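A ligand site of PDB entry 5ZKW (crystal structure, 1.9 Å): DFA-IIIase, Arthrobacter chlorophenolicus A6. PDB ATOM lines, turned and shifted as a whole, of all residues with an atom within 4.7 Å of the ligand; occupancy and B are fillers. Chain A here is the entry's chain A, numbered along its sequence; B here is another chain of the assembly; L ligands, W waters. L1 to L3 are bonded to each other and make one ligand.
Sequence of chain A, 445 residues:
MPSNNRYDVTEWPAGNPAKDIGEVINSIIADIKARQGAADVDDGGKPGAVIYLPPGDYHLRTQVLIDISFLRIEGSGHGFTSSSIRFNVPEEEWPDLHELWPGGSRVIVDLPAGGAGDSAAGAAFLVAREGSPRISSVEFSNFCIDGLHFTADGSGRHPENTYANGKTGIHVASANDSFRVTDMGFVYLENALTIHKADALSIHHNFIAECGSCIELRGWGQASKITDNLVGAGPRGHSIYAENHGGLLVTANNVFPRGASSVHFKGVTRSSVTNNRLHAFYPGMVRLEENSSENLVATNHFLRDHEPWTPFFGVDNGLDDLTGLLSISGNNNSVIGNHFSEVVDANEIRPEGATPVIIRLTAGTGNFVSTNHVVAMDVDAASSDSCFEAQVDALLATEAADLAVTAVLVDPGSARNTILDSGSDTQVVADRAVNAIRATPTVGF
Residues that only touch the ligand: Phe 281, Gln 222 of chain B, Trp 309, Asp 199 of chain B, Ile 85, Pro 308, Phe 256 and Asp 177 of chain B. Hydrophobic or aromatic side chains that line the ligand: Ile 85, Phe 256, Pro 257, Phe 281, Pro 308 and Trp 309. 13 residues have an atom within 4 Å of the ligand: Ser 84, Ile 85, Glu 210, Phe 256, Pro 257, Arg 258, Phe 281, Pro 308, Trp 309, Arg 134 of chain B, Asp 177 of chain B, Asp 199 of chain B and Gln 222 of chain B.
Water W12 lies within hydrogen-bond range of the side-chain hydroxyl of Tyr 163 (2.7 Å), an oxygen (O3) of LIG L1 (2.7 Å), the backbone carbonyl oxygen of Ala 233 (2.8 Å), the backbone NH of Glu 210 (3.4 Å) and the backbone carbonyl oxygen of Gly 232 (3.5 Å). Water W4 lies within hydrogen-bond range of O5 of LIG L1 (2.7 Å), OE2 of Glu 307 (2.8 Å) and NH2 of Arg 258 (3.0 Å). Water W11 bridges the side-chain carboxylate (OD1) of Asp 177 of chain B (2.6 Å) and an oxygen (O4) of LG2 L2 (2.8 Å). Water W2 bridges the side-chain amide nitrogen (NE2) of Gln 222 of chain B (2.7 Å) and an oxygen (O6) of LG2 L2 (2.9 Å). Water W6 bridges OD1 of Asp 199 of chain B (2.5 Å) and O5 of LG3 L3 (3.2 Å).
O3 of LIG L1 is in hydrogen-bond range of O of Pro 257 (2.6 Å). OE2 of Glu 210 sits at hydrogen-bond distance from O2 of LIG L1 (2.6 Å). The side-chain hydroxyl (OG) of Ser 84 sits at hydrogen-bond distance from an oxygen (O1) of LIG L1 (2.7 Å). NH1 of Arg 258 lies within hydrogen-bond range of O1 of LIG L1, 2.9 Å away. NH1 of Arg 134 of chain B is in hydrogen-bond range of O4 of LG2 L2 (3.0 Å).
The backbone carbonyl oxygen of Gly 232 lies within hydrogen-bond range of the backbone NH of Glu 210. The side-chain hydroxyl (OG) of Ser 82 lies within hydrogen-bond range of the side-chain carboxylate (OE2) of Glu 210, 2.6 Å away. The backbone NH (N) of Arg 258 sits at hydrogen-bond distance from the backbone carbonyl oxygen (O) of Ala 233. The guanidinium group of Arg 258 lies within salt-bridge range of the side-chain carboxylate of Glu 307, 2.9 Å away. OD2 of Asp 199 of chain B lies within salt-bridge range of NH1 of Arg 134 of chain B (2.8 Å). The side-chain carboxylate of Asp 177 of chain B is in salt-bridge range of the guanidinium group of Arg 134 of chain B, 3.7 Å away. The side-chain carboxylate (OD1) of Asp 199 of chain B sits at hydrogen-bond distance from the backbone NH (N) of Gln 222 of chain B. The side-chain carboxylate (OE2) of Glu 307 sits at hydrogen-bond distance from the backbone NH (N) of Trp 309 (3.0 Å).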
ATOM      1  N   SER A  82     -15.403 -15.779   5.805  1.00  0.00           N
ATOM      2  CA  SER A  82     -14.638 -17.007   5.966  1.00  0.00           C
ATOM      3  C   SER A  82     -14.656 -17.456   7.429  1.00  0.00           C
ATOM      4  O   SER A  82     -13.810 -17.052   8.233  1.00  0.00           O
ATOM      5  CB  SER A  82     -13.190 -16.847   5.493  1.00  0.00           C
ATOM      6  OG  SER A  82     -12.512 -18.090   5.644  1.00  0.00           O
ATOM      7  N   SER A  84     -13.883 -20.401   8.203  1.00  0.00           N
ATOM      8  CA  SER A  84     -12.640 -21.168   8.281  1.00  0.00           C
ATOM      9  C   SER A  84     -11.489 -20.320   8.817  1.00  0.00           C
ATOM     10  O   SER A  84     -10.793 -20.736   9.740  1.00  0.00           O
ATOM     11  CB  SER A  84     -12.271 -21.791   6.938  1.00  0.00           C
ATOM     12  OG  SER A  84     -11.004 -22.430   6.972  1.00  0.00           O
ATOM     13  N   ILE A  85     -11.292 -19.133   8.251  1.00  0.00           N
ATOM     14  CA  ILE A  85     -10.238 -18.213   8.737  1.00  0.00           C
ATOM     15  C   ILE A  85     -10.521 -17.860  10.202  1.00  0.00           C
ATOM     16  O   ILE A  85      -9.619 -17.997  11.041  1.00  0.00           O
ATOM     17  CB  ILE A  85     -10.070 -16.960   7.835  1.00  0.00           C
ATOM     18  CG1 ILE A  85      -9.311 -17.363   6.554  1.00  0.00           C
ATOM     19  CG2 ILE A  85      -9.304 -15.838   8.524  1.00  0.00           C
ATOM     20  CD1 ILE A  85      -9.335 -16.344   5.433  1.00  0.00           C
ATOM     21  N   TYR A 163     -14.780 -30.291   8.062  1.00  0.00           N
ATOM     22  CA  TYR A 163     -15.821 -30.260   7.039  1.00  0.00           C
ATOM     23  C   TYR A 163     -16.953 -31.285   7.292  1.00  0.00           C
ATOM     24  O   TYR A 163     -17.672 -31.644   6.364  1.00  0.00           O
ATOM     25  CB  TYR A 163     -15.234 -30.425   5.624  1.00  0.00           C
ATOM     26  CG  TYR A 163     -14.406 -29.283   5.110  1.00  0.00           C
ATOM     27  CD1 TYR A 163     -13.057 -29.216   5.382  1.00  0.00           C
ATOM     28  CD2 TYR A 163     -14.973 -28.281   4.314  1.00  0.00           C
ATOM     29  CE1 TYR A 163     -12.280 -28.177   4.902  1.00  0.00           C
ATOM     30  CE2 TYR A 163     -14.205 -27.255   3.809  1.00  0.00           C
ATOM     31  CZ  TYR A 163     -12.861 -27.192   4.108  1.00  0.00           C
ATOM     32  OH  TYR A 163     -12.079 -26.175   3.619  1.00  0.00           O
ATOM     33  N   GLU A 210     -16.259 -23.271   1.590  1.00  0.00           N
ATOM     34  CA  GLU A 210     -16.082 -23.842   2.953  1.00  0.00           C
ATOM     35  C   GLU A 210     -17.203 -24.812   3.303  1.00  0.00           C
ATOM     36  O   GLU A 210     -17.740 -24.800   4.407  1.00  0.00           O
ATOM     37  CB  GLU A 210     -15.889 -22.705   3.952  1.00  0.00           C
ATOM     38  CG  GLU A 210     -14.703 -21.844   3.539  1.00  0.00           C
ATOM     39  CD  GLU A 210     -14.374 -20.699   4.475  1.00  0.00           C
ATOM     40  OE1 GLU A 210     -15.040 -20.499   5.497  1.00  0.00           O
ATOM     41  OE2 GLU A 210     -13.399 -19.982   4.151  1.00  0.00           O
ATOM     42  N   GLY A 232     -15.633 -23.582  -3.569  1.00  0.00           N
ATOM     43  CA  GLY A 232     -14.511 -24.148  -2.854  1.00  0.00           C
ATOM     44  C   GLY A 232     -14.984 -25.158  -1.832  1.00  0.00           C
ATOM     45  O   GLY A 232     -15.720 -24.806  -0.925  1.00  0.00           O
ATOM     46  N   ALA A 233     -14.531 -26.393  -1.965  1.00  0.00           N
ATOM     47  CA  ALA A 233     -15.033 -27.486  -1.134  1.00  0.00           C
ATOM     48  C   ALA A 233     -13.962 -27.991  -0.144  1.00  0.00           C
ATOM     49  O   ALA A 233     -12.982 -27.286   0.140  1.00  0.00           O
ATOM     50  CB  ALA A 233     -15.574 -28.604  -2.031  1.00  0.00           C
ATOM     51  N   PHE A 256     -11.872 -23.023  -6.687  1.00  0.00           N
ATOM     52  CA  PHE A 256     -10.660 -22.866  -5.898  1.00  0.00           C
ATOM     53  C   PHE A 256     -10.633 -24.033  -4.885  1.00  0.00           C
ATOM     54  O   PHE A 256     -11.601 -24.790  -4.811  1.00  0.00           O
ATOM     55  CB  PHE A 256     -10.577 -21.478  -5.253  1.00  0.00           C
ATOM     56  CG  PHE A 256     -11.844 -21.010  -4.586  1.00  0.00           C
ATOM     57  CD1 PHE A 256     -12.083 -21.265  -3.237  1.00  0.00           C
ATOM     58  CD2 PHE A 256     -12.780 -20.241  -5.306  1.00  0.00           C
ATOM     59  CE1 PHE A 256     -13.247 -20.802  -2.619  1.00  0.00           C
ATOM     60  CE2 PHE A 256     -13.947 -19.789  -4.697  1.00  0.00           C
ATOM     61  CZ  PHE A 256     -14.171 -20.068  -3.348  1.00  0.00           C
ATOM     62  N   PRO A 257      -9.522 -24.215  -4.161  1.00  0.00           N
ATOM     63  CA  PRO A 257      -9.443 -25.362  -3.251  1.00  0.00           C
ATOM     64  C   PRO A 257     -10.487 -25.317  -2.129  1.00  0.00           C
ATOM     65  O   PRO A 257     -11.066 -24.263  -1.905  1.00  0.00           O
ATOM     66  CB  PRO A 257      -8.008 -25.261  -2.699  1.00  0.00           C
ATOM     67  CG  PRO A 257      -7.254 -24.596  -3.815  1.00  0.00           C
ATOM     68  CD  PRO A 257      -8.214 -23.543  -4.281  1.00  0.00           C
ATOM     69  N   ARG A 258     -10.736 -26.415  -1.407  1.00  0.00           N
ATOM     70  CA  ARG A 258      -9.880 -27.613  -1.385  1.00  0.00           C
ATOM     71  C   ARG A 258     -10.685 -28.905  -1.460  1.00  0.00           C
ATOM     72  O   ARG A 258     -10.473 -29.848  -0.680  1.00  0.00           O
ATOM     73  CB  ARG A 258      -9.005 -27.600  -0.130  1.00  0.00           C
ATOM     74  CG  ARG A 258      -9.752 -27.472   1.193  1.00  0.00           C
ATOM     75  CD  ARG A 258      -8.831 -27.580   2.395  1.00  0.00           C
ATOM     76  NE  ARG A 258      -7.904 -26.446   2.498  1.00  0.00           N
ATOM     77  CZ  ARG A 258      -8.228 -25.216   2.899  1.00  0.00           C
ATOM     78  NH1 ARG A 258      -9.451 -24.891   3.298  1.00  0.00           N
ATOM     79  NH2 ARG A 258      -7.302 -24.268   2.918  1.00  0.00           N
ATOM     80  N   PHE A 281      -5.195 -28.081  -4.749  1.00  0.00           N
ATOM     81  CA  PHE A 281      -3.981 -28.390  -4.004  1.00  0.00           C
ATOM     82  C   PHE A 281      -3.620 -29.876  -4.086  1.00  0.00           C
ATOM     83  O   PHE A 281      -2.608 -30.301  -3.493  1.00  0.00           O
ATOM     84  CB  PHE A 281      -4.121 -28.001  -2.517  1.00  0.00           C
ATOM     85  CG  PHE A 281      -4.230 -26.520  -2.261  1.00  0.00           C
ATOM     86  CD1 PHE A 281      -3.516 -25.576  -3.004  1.00  0.00           C
ATOM     87  CD2 PHE A 281      -5.009 -26.057  -1.192  1.00  0.00           C
ATOM     88  CE1 PHE A 281      -3.620 -24.221  -2.728  1.00  0.00           C
ATOM     89  CE2 PHE A 281      -5.113 -24.718  -0.919  1.00  0.00           C
ATOM     90  CZ  PHE A 281      -4.421 -23.789  -1.683  1.00  0.00           C
ATOM     91  N   GLU A 307      -0.922 -26.568  -0.877  1.00  0.00           N
ATOM     92  CA  GLU A 307      -1.575 -25.850   0.235  1.00  0.00           C
ATOM     93  C   GLU A 307      -0.591 -24.957   0.959  1.00  0.00           C
ATOM     94  O   GLU A 307       0.421 -25.473   1.459  1.00  0.00           O
ATOM     95  CB  GLU A 307      -2.132 -26.873   1.233  1.00  0.00           C
ATOM     96  CG  GLU A 307      -2.724 -26.315   2.514  1.00  0.00           C
ATOM     97  CD  GLU A 307      -3.967 -25.484   2.279  1.00  0.00           C
ATOM     98  OE1 GLU A 307      -5.041 -26.083   2.081  1.00  0.00           O
ATOM     99  OE2 GLU A 307      -3.874 -24.237   2.319  1.00  0.00           O
ATOM    100  N   PRO A 308      -0.858 -23.637   1.012  1.00  0.00           N
ATOM    101  CA  PRO A 308       0.086 -22.772   1.725  1.00  0.00           C
ATOM    102  C   PRO A 308      -0.262 -22.548   3.204  1.00  0.00           C
ATOM    103  O   PRO A 308       0.586 -22.029   3.945  1.00  0.00           O
ATOM    104  CB  PRO A 308      -0.045 -21.459   0.961  1.00  0.00           C
ATOM    105  CG  PRO A 308      -1.476 -21.424   0.559  1.00  0.00           C
ATOM    106  CD  PRO A 308      -1.861 -22.837   0.278  1.00  0.00           C
ATOM    107  N   TRP A 309      -1.472 -22.897   3.626  1.00  0.00           N
ATOM    108  CA  TRP A 309      -2.001 -22.475   4.920  1.00  0.00           C
ATOM    109  C   TRP A 309      -1.789 -23.554   5.993  1.00  0.00           C
ATOM    110  O   TRP A 309      -2.297 -24.661   5.864  1.00  0.00           O
ATOM    111  CB  TRP A 309      -3.479 -22.104   4.776  1.00  0.00           C
ATOM    112  CG  TRP A 309      -4.053 -21.351   5.920  1.00  0.00           C
ATOM    113  CD1 TRP A 309      -3.418 -20.422   6.705  1.00  0.00           C
ATOM    114  CD2 TRP A 309      -5.391 -21.437   6.394  1.00  0.00           C
ATOM    115  NE1 TRP A 309      -4.288 -19.940   7.652  1.00  0.00           N
ATOM    116  CE2 TRP A 309      -5.508 -20.554   7.484  1.00  0.00           C
ATOM    117  CE3 TRP A 309      -6.516 -22.203   6.019  1.00  0.00           C
ATOM    118  CZ2 TRP A 309      -6.696 -20.392   8.208  1.00  0.00           C
ATOM    119  CZ3 TRP A 309      -7.686 -22.046   6.730  1.00  0.00           C
ATOM    120  CH2 TRP A 309      -7.776 -21.144   7.813  1.00  0.00           C
ATOM    121  N   PHE A 312      -4.045 -26.683   7.225  1.00  0.00           N
ATOM    122  CA  PHE A 312      -4.319 -27.774   6.277  1.00  0.00           C
ATOM    123  C   PHE A 312      -3.052 -28.355   5.660  1.00  0.00           C
ATOM    124  O   PHE A 312      -3.126 -29.140   4.718  1.00  0.00           O
ATOM    125  CB  PHE A 312      -5.306 -27.287   5.205  1.00  0.00           C
ATOM    126  CG  PHE A 312      -6.688 -27.098   5.753  1.00  0.00           C
ATOM    127  CD1 PHE A 312      -7.540 -28.170   5.860  1.00  0.00           C
ATOM    128  CD2 PHE A 312      -7.096 -25.858   6.213  1.00  0.00           C
ATOM    129  CE1 PHE A 312      -8.810 -28.007   6.381  1.00  0.00           C
ATOM    130  CE2 PHE A 312      -8.366 -25.678   6.736  1.00  0.00           C
ATOM    131  CZ  PHE A 312      -9.222 -26.760   6.834  1.00  0.00           C
ATOM    132  N   ARG B 134     -11.202  -9.109   6.562  1.00  0.00           N
ATOM    133  CA  ARG B 134     -11.524  -8.375   5.335  1.00  0.00           C
ATOM    134  C   ARG B 134     -13.003  -8.057   5.283  1.00  0.00           C
ATOM    135  O   ARG B 134     -13.849  -8.917   5.617  1.00  0.00           O
ATOM    136  CB  ARG B 134     -11.169  -9.179   4.080  1.00  0.00           C
ATOM    137  CG  ARG B 134      -9.685  -9.357   3.811  1.00  0.00           C
ATOM    138  CD  ARG B 134      -9.439 -10.498   2.837  1.00  0.00           C
ATOM    139  NE  ARG B 134      -9.856 -11.783   3.409  1.00  0.00           N
ATOM    140  CZ  ARG B 134      -9.961 -12.946   2.748  1.00  0.00           C
ATOM    141  NH1 ARG B 134      -9.657 -13.033   1.456  1.00  0.00           N
ATOM    142  NH2 ARG B 134     -10.369 -14.039   3.407  1.00  0.00           N
ATOM    143  N   ASP B 177     -13.437  -9.445   0.281  1.00  0.00           N
ATOM    144  CA  ASP B 177     -13.706 -10.829  -0.048  1.00  0.00           C
ATOM    145  C   ASP B 177     -15.163 -10.991  -0.461  1.00  0.00           C
ATOM    146  O   ASP B 177     -16.050 -10.436   0.182  1.00  0.00           O
ATOM    147  CB  ASP B 177     -13.431 -11.715   1.178  1.00  0.00           C
ATOM    148  CG  ASP B 177     -13.438 -13.188   0.874  1.00  0.00           C
ATOM    149  OD1 ASP B 177     -13.117 -13.574  -0.284  1.00  0.00           O
ATOM    150  OD2 ASP B 177     -13.727 -13.977   1.807  1.00  0.00           O
ATOM    151  N   ASP B 199     -10.386 -10.385  -3.353  1.00  0.00           N
ATOM    152  CA  ASP B 199     -10.411 -11.842  -3.397  1.00  0.00           C
ATOM    153  C   ASP B 199     -11.826 -12.328  -3.710  1.00  0.00           C
ATOM    154  O   ASP B 199     -12.803 -11.841  -3.115  1.00  0.00           O
ATOM    155  CB  ASP B 199      -9.965 -12.453  -2.066  1.00  0.00           C
ATOM    156  CG  ASP B 199      -8.530 -12.151  -1.739  1.00  0.00           C
ATOM    157  OD1 ASP B 199      -7.663 -12.278  -2.636  1.00  0.00           O
ATOM    158  OD2 ASP B 199      -8.265 -11.762  -0.566  1.00  0.00           O
ATOM    159  N   GLN B 222      -7.101 -12.393  -6.062  1.00  0.00           N
ATOM    160  CA  GLN B 222      -7.128 -13.821  -6.312  1.00  0.00           C
ATOM    161  C   GLN B 222      -8.532 -14.326  -6.575  1.00  0.00           C
ATOM    162  O   GLN B 222      -9.498 -13.832  -5.991  1.00  0.00           O
ATOM    163  CB  GLN B 222      -6.510 -14.560  -5.121  1.00  0.00           C
ATOM    164  CG  GLN B 222      -6.459 -16.076  -5.211  1.00  0.00           C
ATOM    165  CD  GLN B 222      -5.580 -16.616  -6.324  1.00  0.00           C
ATOM    166  OE1 GLN B 222      -4.510 -16.082  -6.636  1.00  0.00           O
ATOM    167  NE2 GLN B 222      -6.026 -17.703  -6.917  1.00  0.00           N
ATOM    168  N   ALA B 223      -8.627 -15.332  -7.437  1.00  0.00           N
ATOM    169  CA  ALA B 223      -9.863 -16.101  -7.622  1.00  0.00           C
ATOM    170  C   ALA B 223     -11.086 -15.246  -7.944  1.00  0.00           C
ATOM    171  O   ALA B 223     -12.177 -15.533  -7.477  1.00  0.00           O
ATOM    172  CB  ALA B 223     -10.124 -16.948  -6.374  1.00  0.00           C
HETATM  173  C1  LIG L   1      -9.882 -21.009   3.925  1.00  0.00           C
HETATM  174  C2  LIG L   1      -9.954 -21.010   2.399  1.00  0.00           C
HETATM  175  C3  LIG L   1     -11.340 -21.369   1.891  1.00  0.00           C
HETATM  176  C4  LIG L   1     -11.050 -21.992   0.520  1.00  0.00           C
HETATM  177  C5  LIG L   1      -9.617 -22.522   0.627  1.00  0.00           C
HETATM  178  C6  LIG L   1      -8.761 -22.044  -0.541  1.00  0.00           C
HETATM  179  O1  LIG L   1     -10.127 -22.321   4.429  1.00  0.00           O
HETATM  180  O2  LIG L   1     -12.218 -20.228   1.821  1.00  0.00           O
HETATM  181  O3  LIG L   1     -12.013 -23.009   0.166  1.00  0.00           O
HETATM  182  O4  LIG L   1      -9.103 -22.036   1.871  1.00  0.00           O
HETATM  183  O5  LIG L   1      -7.409 -22.507  -0.482  1.00  0.00           O
HETATM  184  C1  LG2 L   2      -8.249 -19.288   1.995  1.00  0.00           C
HETATM  185  C2  LG2 L   2      -7.898 -18.224   0.974  1.00  0.00           C
HETATM  186  C3  LG2 L   2      -8.705 -16.948   1.175  1.00  0.00           C
HETATM  187  C4  LG2 L   2      -8.704 -16.383  -0.238  1.00  0.00           C
HETATM  188  C5  LG2 L   2      -8.903 -17.631  -1.079  1.00  0.00           C
HETATM  189  C6  LG2 L   2      -8.394 -17.542  -2.514  1.00  0.00           C
HETATM  190  O1  LG2 L   2      -9.596 -19.748   1.827  1.00  0.00           O
HETATM  191  O2  LG2 L   2      -6.510 -17.897   1.094  1.00  0.00           O
HETATM  192  O3  LG2 L   2      -8.119 -16.074   2.146  1.00  0.00           O
HETATM  193  O4  LG2 L   2      -9.733 -15.410  -0.386  1.00  0.00           O
HETATM  194  O5  LG2 L   2      -8.220 -18.664  -0.361  1.00  0.00           O
HETATM  195  O6  LG2 L   2      -8.509 -18.796  -3.190  1.00  0.00           O
HETATM  196  C1  LG3 L   3      -5.619 -18.640   0.259  1.00  0.00           C
HETATM  197  C2  LG3 L   3      -4.291 -18.947   0.945  1.00  0.00           C
HETATM  198  C3  LG3 L   3      -3.529 -17.674   1.271  1.00  0.00           C
HETATM  199  C4  LG3 L   3      -3.300 -16.849   0.015  1.00  0.00           C
HETATM  200  C5  LG3 L   3      -4.571 -16.695  -0.821  1.00  0.00           C
HETATM  201  C6  LG3 L   3      -4.140 -16.377  -2.259  1.00  0.00           C
HETATM  202  O1  LG3 L   3      -4.523 -19.705   2.138  1.00  0.00           O
HETATM  203  O2  LG3 L   3      -2.222 -18.033   1.750  1.00  0.00           O
HETATM  204  O3  LG3 L   3      -2.796 -15.563   0.400  1.00  0.00           O
HETATM  205  O4  LG3 L   3      -5.394 -17.862  -0.911  1.00  0.00           O
HETATM  206  O5  LG3 L   3      -4.644 -15.082  -2.504  1.00  0.00           O
HETATM  207  O   HOH W   1      -6.457 -20.900  -2.575  1.00  0.00           O
HETATM  208  O   HOH W   2      -7.581 -19.675  -5.806  1.00  0.00           O
HETATM  209  O   HOH W   3     -11.505 -17.952  -3.124  1.00  0.00           O
HETATM  210  O   HOH W   4      -5.628 -22.167   1.548  1.00  0.00           O
HETATM  211  O   HOH W   5      -5.614 -18.483   4.368  1.00  0.00           O
HETATM  212  O   HOH W   6      -5.225 -11.933  -2.159  1.00  0.00           O
HETATM  213  O   HOH W   7      -6.005 -14.617   2.580  1.00  0.00           O
HETATM  214  O   HOH W   8     -12.912 -18.542  -0.394  1.00  0.00           O
HETATM  215  O   HOH W   9      -3.238 -12.483  -3.704  1.00  0.00           O
HETATM  216  O   HOH W  10      -0.186 -18.142  -0.435  1.00  0.00           O
HETATM  217  O   HOH W  11     -12.470 -16.099  -0.544  1.00  0.00           O
HETATM  218  O   HOH W  12     -13.270 -24.931   1.560  1.00  0.00           O
